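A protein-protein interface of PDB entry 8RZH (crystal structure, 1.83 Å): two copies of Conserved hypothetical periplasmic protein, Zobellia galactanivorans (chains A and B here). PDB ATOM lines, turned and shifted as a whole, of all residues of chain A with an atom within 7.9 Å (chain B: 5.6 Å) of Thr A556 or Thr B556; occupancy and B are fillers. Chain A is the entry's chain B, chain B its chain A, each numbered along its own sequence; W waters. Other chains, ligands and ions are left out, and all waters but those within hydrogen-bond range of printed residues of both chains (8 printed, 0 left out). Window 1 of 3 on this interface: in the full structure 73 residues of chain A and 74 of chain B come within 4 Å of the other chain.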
ATOM      1  N   ASN A 176     -11.787 -32.099 -28.036  1.00  0.00           N
ATOM      2  CA  ASN A 176     -13.044 -32.253 -27.330  1.00  0.00           C
ATOM      3  C   ASN A 176     -13.983 -31.091 -27.616  1.00  0.00           C
ATOM      4  O   ASN A 176     -13.559 -29.938 -27.651  1.00  0.00           O
ATOM      5  CB  ASN A 176     -12.810 -32.294 -25.810  1.00  0.00           C
ATOM      6  CG  ASN A 176     -14.102 -32.156 -25.083  1.00  0.00           C
ATOM      7  OD1 ASN A 176     -14.435 -31.084 -24.566  1.00  0.00           O
ATOM      8  ND2 ASN A 176     -14.920 -33.246 -25.121  1.00  0.00           N
ATOM      9  N   ARG A 179     -13.856 -28.077 -25.142  1.00  0.00           N
ATOM     10  CA  ARG A 179     -12.595 -27.374 -25.363  1.00  0.00           C
ATOM     11  C   ARG A 179     -12.630 -26.582 -26.663  1.00  0.00           C
ATOM     12  O   ARG A 179     -12.107 -25.465 -26.720  1.00  0.00           O
ATOM     13  CB  ARG A 179     -11.432 -28.354 -25.415  1.00  0.00           C
ATOM     14  CG  ARG A 179     -11.279 -29.184 -24.128  1.00  0.00           C
ATOM     15  CD  ARG A 179     -10.853 -28.290 -22.961  1.00  0.00           C
ATOM     16  NE  ARG A 179     -10.667 -29.127 -21.760  1.00  0.00           N
ATOM     17  CZ  ARG A 179     -10.328 -28.674 -20.557  1.00  0.00           C
ATOM     18  NH1 ARG A 179     -10.000 -27.390 -20.375  1.00  0.00           N
ATOM     19  NH2 ARG A 179     -10.210 -29.549 -19.560  1.00  0.00           N
ATOM     20  N   LYS A 182     -14.617 -23.308 -26.459  1.00  0.00           N
ATOM     21  CA  LYS A 182     -13.875 -22.266 -25.753  1.00  0.00           C
ATOM     22  C   LYS A 182     -12.686 -21.776 -26.561  1.00  0.00           C
ATOM     23  O   LYS A 182     -12.325 -20.583 -26.501  1.00  0.00           O
ATOM     24  CB  LYS A 182     -13.369 -22.801 -24.395  1.00  0.00           C
ATOM     25  CG  LYS A 182     -14.555 -23.005 -23.401  1.00  0.00           C
ATOM     26  CD  LYS A 182     -14.020 -23.433 -21.991  1.00  0.00           C
ATOM     27  CE  LYS A 182     -13.636 -24.938 -22.058  1.00  0.00           C
ATOM     28  NZ  LYS A 182     -13.031 -25.379 -20.721  1.00  0.00           N
ATOM     29  N   TYR A 518       2.615 -24.644 -14.354  1.00  0.00           N
ATOM     30  CA  TYR A 518       1.531 -23.838 -14.942  1.00  0.00           C
ATOM     31  C   TYR A 518       0.666 -23.235 -13.841  1.00  0.00           C
ATOM     32  O   TYR A 518       0.306 -23.946 -12.891  1.00  0.00           O
ATOM     33  CB  TYR A 518       0.618 -24.719 -15.878  1.00  0.00           C
ATOM     34  CG  TYR A 518       1.446 -25.195 -17.022  1.00  0.00           C
ATOM     35  CD1 TYR A 518       1.673 -24.365 -18.113  1.00  0.00           C
ATOM     36  CD2 TYR A 518       2.139 -26.412 -16.951  1.00  0.00           C
ATOM     37  CE1 TYR A 518       2.491 -24.776 -19.171  1.00  0.00           C
ATOM     38  CE2 TYR A 518       3.001 -26.801 -17.964  1.00  0.00           C
ATOM     39  CZ  TYR A 518       3.193 -25.964 -19.053  1.00  0.00           C
ATOM     40  OH  TYR A 518       4.058 -26.300 -20.073  1.00  0.00           O
ATOM     41  N   LEU A 519       0.276 -21.961 -13.995  1.00  0.00           N
ATOM     42  CA  LEU A 519      -0.850 -21.450 -13.209  1.00  0.00           C
ATOM     43  C   LEU A 519      -2.116 -22.228 -13.565  1.00  0.00           C
ATOM     44  O   LEU A 519      -2.249 -22.759 -14.671  1.00  0.00           O
ATOM     45  CB  LEU A 519      -1.141 -19.980 -13.512  1.00  0.00           C
ATOM     46  CG  LEU A 519      -0.126 -18.912 -13.128  1.00  0.00           C
ATOM     47  CD1 LEU A 519      -0.798 -17.511 -13.349  1.00  0.00           C
ATOM     48  CD2 LEU A 519       0.274 -19.104 -11.682  1.00  0.00           C
ATOM     49  N   GLU A 520      -3.075 -22.257 -12.628  1.00  0.00           N
ATOM     50  CA  GLU A 520      -4.361 -22.881 -12.950  1.00  0.00           C
ATOM     51  C   GLU A 520      -5.191 -22.002 -13.876  1.00  0.00           C
ATOM     52  O   GLU A 520      -5.776 -22.491 -14.846  1.00  0.00           O
ATOM     53  CB  GLU A 520      -5.139 -23.180 -11.651  1.00  0.00           C
ATOM     54  CG  GLU A 520      -4.491 -24.301 -10.843  1.00  0.00           C
ATOM     55  CD  GLU A 520      -4.991 -24.294  -9.393  1.00  0.00           C
ATOM     56  OE1 GLU A 520      -6.223 -24.466  -9.226  1.00  0.00           O
ATOM     57  OE2 GLU A 520      -4.185 -23.990  -8.463  1.00  0.00           O
ATOM     58  N   ASP A 521      -5.305 -20.727 -13.555  1.00  0.00           N
ATOM     59  CA  ASP A 521      -6.036 -19.741 -14.354  1.00  0.00           C
ATOM     60  C   ASP A 521      -4.998 -18.792 -14.939  1.00  0.00           C
ATOM     61  O   ASP A 521      -4.222 -18.191 -14.186  1.00  0.00           O
ATOM     62  CB  ASP A 521      -7.028 -18.966 -13.485  1.00  0.00           C
ATOM     63  CG  ASP A 521      -8.060 -19.883 -12.843  1.00  0.00           C
ATOM     64  OD1 ASP A 521      -8.607 -20.760 -13.561  1.00  0.00           O
ATOM     65  OD2 ASP A 521      -8.289 -19.741 -11.618  1.00  0.00           O
ATOM     66  N   GLN A 549       0.494 -25.378  -4.640  1.00  0.00           N
ATOM     67  CA  GLN A 549      -0.908 -24.965  -4.769  1.00  0.00           C
ATOM     68  C   GLN A 549      -1.693 -25.836  -5.740  1.00  0.00           C
ATOM     69  O   GLN A 549      -2.944 -25.887  -5.666  1.00  0.00           O
ATOM     70  CB  GLN A 549      -1.018 -23.507  -5.267  1.00  0.00           C
ATOM     71  CG  GLN A 549      -0.802 -22.439  -4.195  1.00  0.00           C
ATOM     72  CD  GLN A 549       0.672 -22.101  -4.009  1.00  0.00           C
ATOM     73  OE1 GLN A 549       1.542 -22.717  -4.641  1.00  0.00           O
ATOM     74  NE2 GLN A 549       0.957 -21.093  -3.183  1.00  0.00           N
ATOM     75  N   ASP A 550      -0.998 -26.528  -6.650  1.00  0.00           N
ATOM     76  CA  ASP A 550      -1.637 -27.317  -7.705  1.00  0.00           C
ATOM     77  C   ASP A 550      -0.966 -28.679  -7.744  1.00  0.00           C
ATOM     78  O   ASP A 550      -0.410 -29.077  -8.761  1.00  0.00           O
ATOM     79  CB  ASP A 550      -1.481 -26.593  -9.044  1.00  0.00           C
ATOM     80  CG  ASP A 550      -2.242 -27.274 -10.170  1.00  0.00           C
ATOM     81  OD1 ASP A 550      -3.192 -28.024  -9.880  1.00  0.00           O
ATOM     82  OD2 ASP A 550      -1.876 -27.079 -11.337  1.00  0.00           O
ATOM     83  N   PRO A 551      -0.967 -29.412  -6.631  1.00  0.00           N
ATOM     84  CA  PRO A 551      -0.147 -30.623  -6.531  1.00  0.00           C
ATOM     85  C   PRO A 551      -0.780 -31.767  -7.310  1.00  0.00           C
ATOM     86  O   PRO A 551      -1.903 -31.679  -7.790  1.00  0.00           O
ATOM     87  CB  PRO A 551      -0.161 -30.922  -5.017  1.00  0.00           C
ATOM     88  CG  PRO A 551      -1.524 -30.439  -4.582  1.00  0.00           C
ATOM     89  CD  PRO A 551      -1.744 -29.169  -5.404  1.00  0.00           C
ATOM     90  N   ASP A 552      -0.067 -32.893  -7.346  1.00  0.00           N
ATOM     91  CA  ASP A 552      -0.561 -34.001  -8.160  1.00  0.00           C
ATOM     92  C   ASP A 552      -1.732 -34.736  -7.531  1.00  0.00           C
ATOM     93  O   ASP A 552      -2.432 -35.445  -8.260  1.00  0.00           O
ATOM     94  CB  ASP A 552       0.612 -34.943  -8.466  1.00  0.00           C
ATOM     95  CG  ASP A 552       1.660 -34.254  -9.347  1.00  0.00           C
ATOM     96  OD1 ASP A 552       1.249 -33.335 -10.109  1.00  0.00           O
ATOM     97  OD2 ASP A 552       2.871 -34.590  -9.275  1.00  0.00           O
ATOM     98  N   ASN A 553      -2.030 -34.485  -6.244  1.00  0.00           N
ATOM     99  CA  ASN A 553      -3.206 -35.069  -5.598  1.00  0.00           C
ATOM    100  C   ASN A 553      -4.466 -34.206  -5.688  1.00  0.00           C
ATOM    101  O   ASN A 553      -5.522 -34.654  -5.224  1.00  0.00           O
ATOM    102  CB  ASN A 553      -2.924 -35.354  -4.109  1.00  0.00           C
ATOM    103  CG  ASN A 553      -2.257 -34.172  -3.419  1.00  0.00           C
ATOM    104  OD1 ASN A 553      -1.110 -33.858  -3.717  1.00  0.00           O
ATOM    105  ND2 ASN A 553      -2.984 -33.516  -2.506  1.00  0.00           N
ATOM    106  N   GLU A 554      -4.399 -32.994  -6.244  1.00  0.00           N
ATOM    107  CA  GLU A 554      -5.589 -32.164  -6.386  1.00  0.00           C
ATOM    108  C   GLU A 554      -6.070 -32.162  -7.835  1.00  0.00           C
ATOM    109  O   GLU A 554      -5.260 -32.168  -8.774  1.00  0.00           O
ATOM    110  CB  GLU A 554      -5.283 -30.715  -5.945  1.00  0.00           C
ATOM    111  CG  GLU A 554      -5.221 -30.574  -4.398  1.00  0.00           C
ATOM    112  CD  GLU A 554      -6.633 -30.663  -3.826  1.00  0.00           C
ATOM    113  OE1 GLU A 554      -7.541 -29.984  -4.352  1.00  0.00           O
ATOM    114  OE2 GLU A 554      -6.857 -31.480  -2.913  1.00  0.00           O
ATOM    115  N   VAL A 555      -7.394 -32.072  -8.019  1.00  0.00           N
ATOM    116  CA  VAL A 555      -7.981 -32.010  -9.359  1.00  0.00           C
ATOM    117  C   VAL A 555      -8.210 -30.538  -9.668  1.00  0.00           C
ATOM    118  O   VAL A 555      -8.946 -29.850  -8.946  1.00  0.00           O
ATOM    119  CB  VAL A 555      -9.308 -32.786  -9.431  1.00  0.00           C
ATOM    120  CG1 VAL A 555      -9.880 -32.715 -10.857  1.00  0.00           C
ATOM    121  CG2 VAL A 555      -9.088 -34.273  -8.966  1.00  0.00           C
ATOM    122  N   THR A 556      -7.577 -30.044 -10.729  1.00  0.00           N
ATOM    123  CA  THR A 556      -7.630 -28.622 -11.029  1.00  0.00           C
ATOM    124  C   THR A 556      -7.770 -28.414 -12.528  1.00  0.00           C
ATOM    125  O   THR A 556      -7.844 -29.363 -13.314  1.00  0.00           O
ATOM    126  CB  THR A 556      -6.376 -27.894 -10.550  1.00  0.00           C
ATOM    127  OG1 THR A 556      -5.269 -28.291 -11.360  1.00  0.00           O
ATOM    128  CG2 THR A 556      -6.065 -28.163  -9.027  1.00  0.00           C
ATOM    129  N   ALA A 557      -7.780 -27.132 -12.927  1.00  0.00           N
ATOM    130  CA  ALA A 557      -7.731 -26.827 -14.352  1.00  0.00           C
ATOM    131  C   ALA A 557      -6.591 -27.549 -15.058  1.00  0.00           C
ATOM    132  O   ALA A 557      -6.695 -27.796 -16.265  1.00  0.00           O
ATOM    133  CB  ALA A 557      -7.584 -25.309 -14.545  1.00  0.00           C
ATOM    134  N   ASN A 558      -5.484 -27.871 -14.353  1.00  0.00           N
ATOM    135  CA  ASN A 558      -4.337 -28.521 -15.011  1.00  0.00           C
ATOM    136  C   ASN A 558      -4.400 -30.048 -14.991  1.00  0.00           C
ATOM    137  O   ASN A 558      -3.459 -30.692 -15.453  1.00  0.00           O
ATOM    138  CB  ASN A 558      -2.999 -28.030 -14.410  1.00  0.00           C
ATOM    139  CG  ASN A 558      -2.746 -26.546 -14.760  1.00  0.00           C
ATOM    140  OD1 ASN A 558      -2.982 -26.126 -15.892  1.00  0.00           O
ATOM    141  ND2 ASN A 558      -2.345 -25.764 -13.791  1.00  0.00           N
ATOM    142  N   GLY A 559      -5.480 -30.627 -14.472  1.00  0.00           N
ATOM    143  CA  GLY A 559      -5.730 -32.048 -14.577  1.00  0.00           C
ATOM    144  C   GLY A 559      -5.911 -32.685 -13.216  1.00  0.00           C
ATOM    145  O   GLY A 559      -5.850 -32.037 -12.172  1.00  0.00           O
ATOM    146  N   ASP A 560      -6.178 -33.977 -13.267  1.00  0.00           N
ATOM    147  CA  ASP A 560      -6.218 -34.844 -12.119  1.00  0.00           C
ATOM    148  C   ASP A 560      -4.884 -35.606 -12.044  1.00  0.00           C
ATOM    149  O   ASP A 560      -3.938 -35.316 -12.773  1.00  0.00           O
ATOM    150  CB  ASP A 560      -7.399 -35.775 -12.246  1.00  0.00           C
ATOM    151  CG  ASP A 560      -7.320 -36.663 -13.523  1.00  0.00           C
ATOM    152  OD1 ASP A 560      -6.335 -36.574 -14.295  1.00  0.00           O
ATOM    153  OD2 ASP A 560      -8.296 -37.402 -13.794  1.00  0.00           O
ATOM    154  N   PHE A 561      -4.833 -36.641 -11.214  1.00  0.00           N
ATOM    155  CA  PHE A 561      -3.582 -37.374 -11.061  1.00  0.00           C
ATOM    156  C   PHE A 561      -3.192 -38.045 -12.371  1.00  0.00           C
ATOM    157  O   PHE A 561      -2.006 -38.107 -12.715  1.00  0.00           O
ATOM    158  CB  PHE A 561      -3.699 -38.436  -9.952  1.00  0.00           C
ATOM    159  CG  PHE A 561      -2.399 -39.165  -9.710  1.00  0.00           C
ATOM    160  CD1 PHE A 561      -1.453 -38.604  -8.895  1.00  0.00           C
ATOM    161  CD2 PHE A 561      -2.107 -40.361 -10.369  1.00  0.00           C
ATOM    162  CE1 PHE A 561      -0.209 -39.215  -8.674  1.00  0.00           C
ATOM    163  CE2 PHE A 561      -0.868 -40.990 -10.171  1.00  0.00           C
ATOM    164  CZ  PHE A 561       0.081 -40.400  -9.316  1.00  0.00           C
ATOM    165  N   ILE A 563      -3.647 -37.223 -15.522  1.00  0.00           N
ATOM    166  CA  ILE A 563      -3.064 -36.308 -16.479  1.00  0.00           C
ATOM    167  C   ILE A 563      -1.722 -35.771 -15.972  1.00  0.00           C
ATOM    168  O   ILE A 563      -0.737 -35.675 -16.723  1.00  0.00           O
ATOM    169  CB  ILE A 563      -4.082 -35.177 -16.734  1.00  0.00           C
ATOM    170  CG1 ILE A 563      -5.254 -35.733 -17.546  1.00  0.00           C
ATOM    171  CG2 ILE A 563      -3.405 -33.992 -17.493  1.00  0.00           C
ATOM    172  CD1 ILE A 563      -6.461 -34.809 -17.499  1.00  0.00           C
ATOM    173  N   LYS A 564      -1.662 -35.412 -14.686  1.00  0.00           N
ATOM    174  CA  LYS A 564      -0.443 -34.792 -14.168  1.00  0.00           C
ATOM    175  C   LYS A 564       0.713 -35.794 -14.112  1.00  0.00           C
ATOM    176  O   LYS A 564       1.861 -35.427 -14.385  1.00  0.00           O
ATOM    177  CB  LYS A 564      -0.730 -34.212 -12.786  1.00  0.00           C
ATOM    178  CG  LYS A 564      -1.618 -32.921 -12.883  1.00  0.00           C
ATOM    179  CD  LYS A 564      -2.046 -32.503 -11.437  1.00  0.00           C
ATOM    180  CE  LYS A 564      -2.672 -31.060 -11.452  1.00  0.00           C
ATOM    181  NZ  LYS A 564      -3.294 -30.754 -10.118  1.00  0.00           N
ATOM    182  N   ARG A 567       1.922 -36.133 -17.765  1.00  0.00           N
ATOM    183  CA  ARG A 567       2.639 -34.922 -18.147  1.00  0.00           C
ATOM    184  C   ARG A 567       3.974 -34.817 -17.416  1.00  0.00           C
ATOM    185  O   ARG A 567       4.950 -34.369 -18.004  1.00  0.00           O
ATOM    186  CB  ARG A 567       1.781 -33.662 -17.895  1.00  0.00           C
ATOM    187  CG  ARG A 567       2.379 -32.433 -18.592  1.00  0.00           C
ATOM    188  CD  ARG A 567       1.667 -31.128 -18.224  1.00  0.00           C
ATOM    189  NE  ARG A 567       0.241 -31.124 -18.562  1.00  0.00           N
ATOM    190  CZ  ARG A 567      -0.779 -31.063 -17.700  1.00  0.00           C
ATOM    191  NH1 ARG A 567      -0.621 -30.998 -16.352  1.00  0.00           N
ATOM    192  NH2 ARG A 567      -2.005 -31.049 -18.197  1.00  0.00           N
ATOM    193  N   ARG B 179      -5.109 -25.875  -1.447  1.00  0.00           N
ATOM    194  CA  ARG B 179      -6.314 -25.044  -1.361  1.00  0.00           C
ATOM    195  C   ARG B 179      -6.235 -24.031  -0.215  1.00  0.00           C
ATOM    196  O   ARG B 179      -6.711 -22.891  -0.349  1.00  0.00           O
ATOM    197  CB  ARG B 179      -7.552 -25.923  -1.138  1.00  0.00           C
ATOM    198  CG  ARG B 179      -7.765 -26.966  -2.243  1.00  0.00           C
ATOM    199  CD  ARG B 179      -8.213 -26.329  -3.557  1.00  0.00           C
ATOM    200  NE  ARG B 179      -8.400 -27.412  -4.546  1.00  0.00           N
ATOM    201  CZ  ARG B 179      -8.732 -27.204  -5.802  1.00  0.00           C
ATOM    202  NH1 ARG B 179      -8.988 -25.945  -6.214  1.00  0.00           N
ATOM    203  NH2 ARG B 179      -8.826 -28.250  -6.627  1.00  0.00           N
ATOM    204  N   LYS B 182      -4.087 -20.953  -1.029  1.00  0.00           N
ATOM    205  CA  LYS B 182      -4.762 -20.027  -1.941  1.00  0.00           C
ATOM    206  C   LYS B 182      -5.935 -19.327  -1.253  1.00  0.00           C
ATOM    207  O   LYS B 182      -6.187 -18.134  -1.500  1.00  0.00           O
ATOM    208  CB  LYS B 182      -5.288 -20.756  -3.193  1.00  0.00           C
ATOM    209  CG  LYS B 182      -4.184 -21.265  -4.135  1.00  0.00           C
ATOM    210  CD  LYS B 182      -4.844 -21.950  -5.394  1.00  0.00           C
ATOM    211  CE  LYS B 182      -5.306 -23.397  -5.063  1.00  0.00           C
ATOM    212  NZ  LYS B 182      -5.849 -24.093  -6.344  1.00  0.00           N
ATOM    213  N   GLU B 520     -15.674 -22.211 -14.859  1.00  0.00           N
ATOM    214  CA  GLU B 520     -14.428 -22.842 -14.431  1.00  0.00           C
ATOM    215  C   GLU B 520     -13.515 -21.846 -13.708  1.00  0.00           C
ATOM    216  O   GLU B 520     -12.937 -22.168 -12.660  1.00  0.00           O
ATOM    217  CB  GLU B 520     -13.712 -23.421 -15.654  1.00  0.00           C
ATOM    218  CG  GLU B 520     -14.453 -24.623 -16.230  1.00  0.00           C
ATOM    219  CD  GLU B 520     -13.951 -24.986 -17.615  1.00  0.00           C
ATOM    220  OE1 GLU B 520     -12.751 -25.343 -17.726  1.00  0.00           O
ATOM    221  OE2 GLU B 520     -14.748 -24.858 -18.588  1.00  0.00           O
ATOM    222  N   GLN B 549     -19.434 -26.674 -22.081  1.00  0.00           N
ATOM    223  CA  GLN B 549     -18.008 -26.334 -22.018  1.00  0.00           C
ATOM    224  C   GLN B 549     -17.267 -27.094 -20.923  1.00  0.00           C
ATOM    225  O   GLN B 549     -16.031 -27.230 -20.991  1.00  0.00           O
ATOM    226  CB  GLN B 549     -17.798 -24.838 -21.751  1.00  0.00           C
ATOM    227  CG  GLN B 549     -18.012 -23.929 -22.991  1.00  0.00           C
ATOM    228  CD  GLN B 549     -19.450 -23.602 -23.291  1.00  0.00           C
ATOM    229  OE1 GLN B 549     -20.383 -24.079 -22.601  1.00  0.00           O
ATOM    230  NE2 GLN B 549     -19.668 -22.771 -24.351  1.00  0.00           N
ATOM    231  N   ASP B 550     -17.982 -27.528 -19.899  1.00  0.00           N
ATOM    232  CA  ASP B 550     -17.399 -28.146 -18.705  1.00  0.00           C
ATOM    233  C   ASP B 550     -18.142 -29.450 -18.385  1.00  0.00           C
ATOM    234  O   ASP B 550     -18.722 -29.606 -17.303  1.00  0.00           O
ATOM    235  CB  ASP B 550     -17.500 -27.157 -17.543  1.00  0.00           C
ATOM    236  CG  ASP B 550     -16.789 -27.640 -16.284  1.00  0.00           C
ATOM    237  OD1 ASP B 550     -15.899 -28.512 -16.377  1.00  0.00           O
ATOM    238  OD2 ASP B 550     -17.135 -27.128 -15.191  1.00  0.00           O
ATOM    239  N   GLU B 554     -14.951 -34.118 -18.962  1.00  0.00           N
ATOM    240  CA  GLU B 554     -13.744 -33.309 -19.021  1.00  0.00           C
ATOM    241  C   GLU B 554     -13.208 -33.084 -17.608  1.00  0.00           C
ATOM    242  O   GLU B 554     -13.977 -32.968 -16.646  1.00  0.00           O
ATOM    243  CB  GLU B 554     -14.024 -31.946 -19.715  1.00  0.00           C
ATOM    244  CG  GLU B 554     -13.973 -32.097 -21.308  1.00  0.00           C
ATOM    245  CD  GLU B 554     -12.568 -32.421 -21.819  1.00  0.00           C
ATOM    246  OE1 GLU B 554     -11.578 -31.760 -21.408  1.00  0.00           O
ATOM    247  OE2 GLU B 554     -12.412 -33.408 -22.566  1.00  0.00           O
ATOM    248  N   VAL B 555     -11.897 -32.974 -17.493  1.00  0.00           N
ATOM    249  CA  VAL B 555     -11.270 -32.728 -16.192  1.00  0.00           C
ATOM    250  C   VAL B 555     -10.960 -31.230 -16.103  1.00  0.00           C
ATOM    251  O   VAL B 555     -10.138 -30.722 -16.870  1.00  0.00           O
ATOM    252  CB  VAL B 555      -9.991 -33.555 -16.002  1.00  0.00           C
ATOM    253  CG1 VAL B 555      -9.386 -33.211 -14.604  1.00  0.00           C
ATOM    254  CG2 VAL B 555     -10.310 -35.059 -16.083  1.00  0.00           C
ATOM    255  N   THR B 556     -11.610 -30.516 -15.182  1.00  0.00           N
ATOM    256  CA  THR B 556     -11.473 -29.049 -15.138  1.00  0.00           C
ATOM    257  C   THR B 556     -11.322 -28.574 -13.708  1.00  0.00           C
ATOM    258  O   THR B 556     -11.302 -29.368 -12.752  1.00  0.00           O
ATOM    259  CB  THR B 556     -12.696 -28.332 -15.730  1.00  0.00           C
ATOM    260  OG1 THR B 556     -13.832 -28.529 -14.863  1.00  0.00           O
ATOM    261  CG2 THR B 556     -13.031 -28.869 -17.145  1.00  0.00           C
ATOM    262  N   ALA B 557     -11.272 -27.236 -13.566  1.00  0.00           N
ATOM    263  CA  ALA B 557     -11.242 -26.667 -12.214  1.00  0.00           C
ATOM    264  C   ALA B 557     -12.434 -27.121 -11.372  1.00  0.00           C
ATOM    265  O   ALA B 557     -12.362 -27.066 -10.130  1.00  0.00           O
ATOM    266  CB  ALA B 557     -11.219 -25.126 -12.318  1.00  0.00           C
ATOM    267  N   ASN B 558     -13.534 -27.528 -12.009  1.00  0.00           N
ATOM    268  CA  ASN B 558     -14.729 -27.969 -11.284  1.00  0.00           C
ATOM    269  C   ASN B 558     -14.731 -29.455 -11.021  1.00  0.00           C
ATOM    270  O   ASN B 558     -15.678 -29.966 -10.414  1.00  0.00           O
ATOM    271  CB  ASN B 558     -15.974 -27.549 -12.053  1.00  0.00           C
ATOM    272  CG  ASN B 558     -16.174 -26.048 -11.972  1.00  0.00           C
ATOM    273  OD1 ASN B 558     -15.879 -25.449 -10.925  1.00  0.00           O
ATOM    274  ND2 ASN B 558     -16.675 -25.433 -13.056  1.00  0.00           N
ATOM    275  N   GLY B 559     -13.691 -30.168 -11.436  1.00  0.00           N
ATOM    276  CA  GLY B 559     -13.573 -31.548 -11.008  1.00  0.00           C
ATOM    277  C   GLY B 559     -13.413 -32.492 -12.175  1.00  0.00           C
ATOM    278  O   GLY B 559     -13.440 -32.100 -13.343  1.00  0.00           O
ATOM    279  N   ASP B 560     -13.221 -33.778 -11.827  1.00  0.00           N
ATOM    280  CA  ASP B 560     -13.176 -34.882 -12.780  1.00  0.00           C
ATOM    281  C   ASP B 560     -14.541 -35.586 -12.737  1.00  0.00           C
ATOM    282  O   ASP B 560     -15.491 -35.090 -12.122  1.00  0.00           O
ATOM    283  CB  ASP B 560     -11.990 -35.806 -12.427  1.00  0.00           C
ATOM    284  CG  ASP B 560     -12.121 -36.417 -11.030  1.00  0.00           C
ATOM    285  OD1 ASP B 560     -13.080 -36.107 -10.308  1.00  0.00           O
ATOM    286  OD2 ASP B 560     -11.245 -37.177 -10.615  1.00  0.00           O
ATOM    287  N   LYS B 564     -17.722 -34.677 -10.245  1.00  0.00           N
ATOM    288  CA  LYS B 564     -18.912 -34.117 -10.888  1.00  0.00           C
ATOM    289  C   LYS B 564     -20.104 -35.052 -10.749  1.00  0.00           C
ATOM    290  O   LYS B 564     -21.237 -34.587 -10.605  1.00  0.00           O
ATOM    291  CB  LYS B 564     -18.643 -33.849 -12.350  1.00  0.00           C
ATOM    292  CG  LYS B 564     -17.693 -32.621 -12.537  1.00  0.00           C
ATOM    293  CD  LYS B 564     -17.275 -32.481 -13.997  1.00  0.00           C
ATOM    294  CE  LYS B 564     -16.571 -31.099 -14.220  1.00  0.00           C
ATOM    295  NZ  LYS B 564     -15.943 -31.100 -15.633  1.00  0.00           N
HETATM  296  O   HOH W   1     -13.639 -28.355 -20.902  1.00  0.00           O
HETATM  297  O   HOH W   2      -9.678 -38.717 -11.937  1.00  0.00           O
HETATM  298  O   HOH W   3     -11.190 -23.645 -19.201  1.00  0.00           O
HETATM  299  O   HOH W   4      -7.724 -22.571  -8.127  1.00  0.00           O
HETATM  300  O   HOH W   5      -7.447 -30.857 -17.170  1.00  0.00           O
HETATM  301  O   HOH W   6      -5.436 -26.827  -5.609  1.00  0.00           O
HETATM  302  O   HOH W   7     -11.796 -29.923  -8.712  1.00  0.00           O
HETATM  303  O   HOH W   8     -13.584 -35.642 -23.205  1.00  0.00           O
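Hydrophobic or aromatic side chains of chain B that line the printed part of chain A: Val B555.
Of the 23 printed residues of chain A, 11 touch a printed residue of chain B.
Printed residues of chain A that touch a printed residue of chain B: Asn A176, Arg A179, Lys A182, Glu A520, Gln A549, Glu A554, Val A555, Thr A556, Ala A557, Gly A559 and Asp A560.
Among the printed residues, Asp or Glu carboxylates within 4 Å of a Lys or Arg side-chain nitrogen of the other chain: Arg A179 with Glu B554 (2.8 Å), Lys A182 with Glu B520 (2.8 Å), Glu A520 with Lys B182 (2.7 Å) and Glu A554 with Arg B179 (2.7 Å).
The guanidinium group (NE) of Arg B179 is in salt-bridge range of the side-chain carboxylate (OE1) of Glu A554, 2.7 Å away.
NH2 of Arg B179 is in hydrogen-bond range of O of Val A555 (2.8 Å).
OE2 of Glu A520 lies within salt-bridge range of NZ of Lys B182 (2.7 Å).
The side-chain amino group (NZ) of Lys B182 is in hydrogen-bond range of the backbone carbonyl oxygen (O) of Gln A549, at 3.5 Å.
The side-chain amino group (NZ) of Lys A182 lies within salt-bridge range of the side-chain carboxylate (OE2) of Glu B520, at 2.8 Å.
NE of Arg A179 is in salt-bridge range of OE1 of Glu B554 (2.8 Å).
NH2 of Arg A179 is in hydrogen-bond range of O of Val B555 (2.9 Å).
Thr A556 touches three residues of chain B.
Thr B556 touches just these residues of chain A: Arg A179 (3.8 Å), Thr A556 (3.5 Å) and Ala A557 (3.9 Å).
Of chain A, only Thr A556 (3.8 Å) and Ala A557 (3.6 Å) come within 4 Å of Ala B557.
Of chain A, only Val A555 comes within 4 Å of Gly B559.
Printed residues of chain B within 4 Å of Lys A182: Glu B520 (2.8 Å) and Gln B549 (3.5 Å).
Printed residues of chain A within 4 Å of Val B555: Arg A179, Val A555, Gly A559 and Asp A560.
Asn B558 touches none of the printed residues of chain A.
Asp A552 touches none of the printed residues of chain B.
The nearest residue of chain A that does not touch Thr B556 is Val A555 (4.1 Å).
The nearest printed residue of chain A that does not touch Gln B549 is Arg A179 (4.8 Å).
Water W2 lies within hydrogen-bond range of the side-chain carboxylate of Asp B560 and the side-chain carboxylate of Asp A560.
Water W6 lies within hydrogen-bond range of the backbone carbonyl oxygen (O) of Gln A549, the side-chain amino group (NZ) of Lys B182 and the guanidinium group (NE) of Arg B179.
Water W3 lies within hydrogen-bond range of OE1 of Glu B520 (2.7 Å) and NZ of Lys A182 (3.0 Å).
Arg A179 touches Thr B556, and with the chains exchanged Thr A556 touches Arg B179.
Thr B556 touches its own counterpart, Thr A556.
Thr A556 touches Ala B557, and with the chains exchanged Ala A557 touches Thr B556.
Positions printed for both chains: 179, 182, 520, 549, 550, 554, 555, 556, 557, 558, 559, 560 and 564.
The backbone carbonyl oxygen of Glu B554 lies within hydrogen-bond range of the side-chain amino group of Lys B564 (2.9 Å).
OD1 of Asp A550 lies within hydrogen-bond range of OG1 of Thr A556, at 2.6 Å.
The side-chain amino group of Lys A564 sits at hydrogen-bond distance from the side-chain hydroxyl of Thr A556.
Glu B554 touches Asn A176 (OE2 to CG, 3.3 Å).
CG2 of Thr B556 touches NH2 of Arg A179 (3.8 Å).
O of Gln B549 touches CE of Lys A182, at 3.5 Å.
Val A555 touches Val B555 (CG1 to CG1, 3.8 Å).
Gly B559 touches Val A555 (C to CG1, 3.8 Å).
Val A555 touches Asp B560.
Arg B179 touches Thr A556.
O of Thr B556 touches O of Thr A556, 3.5 Å away.
N of Ala B557 touches N of Ala A557 (3.6 Å).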
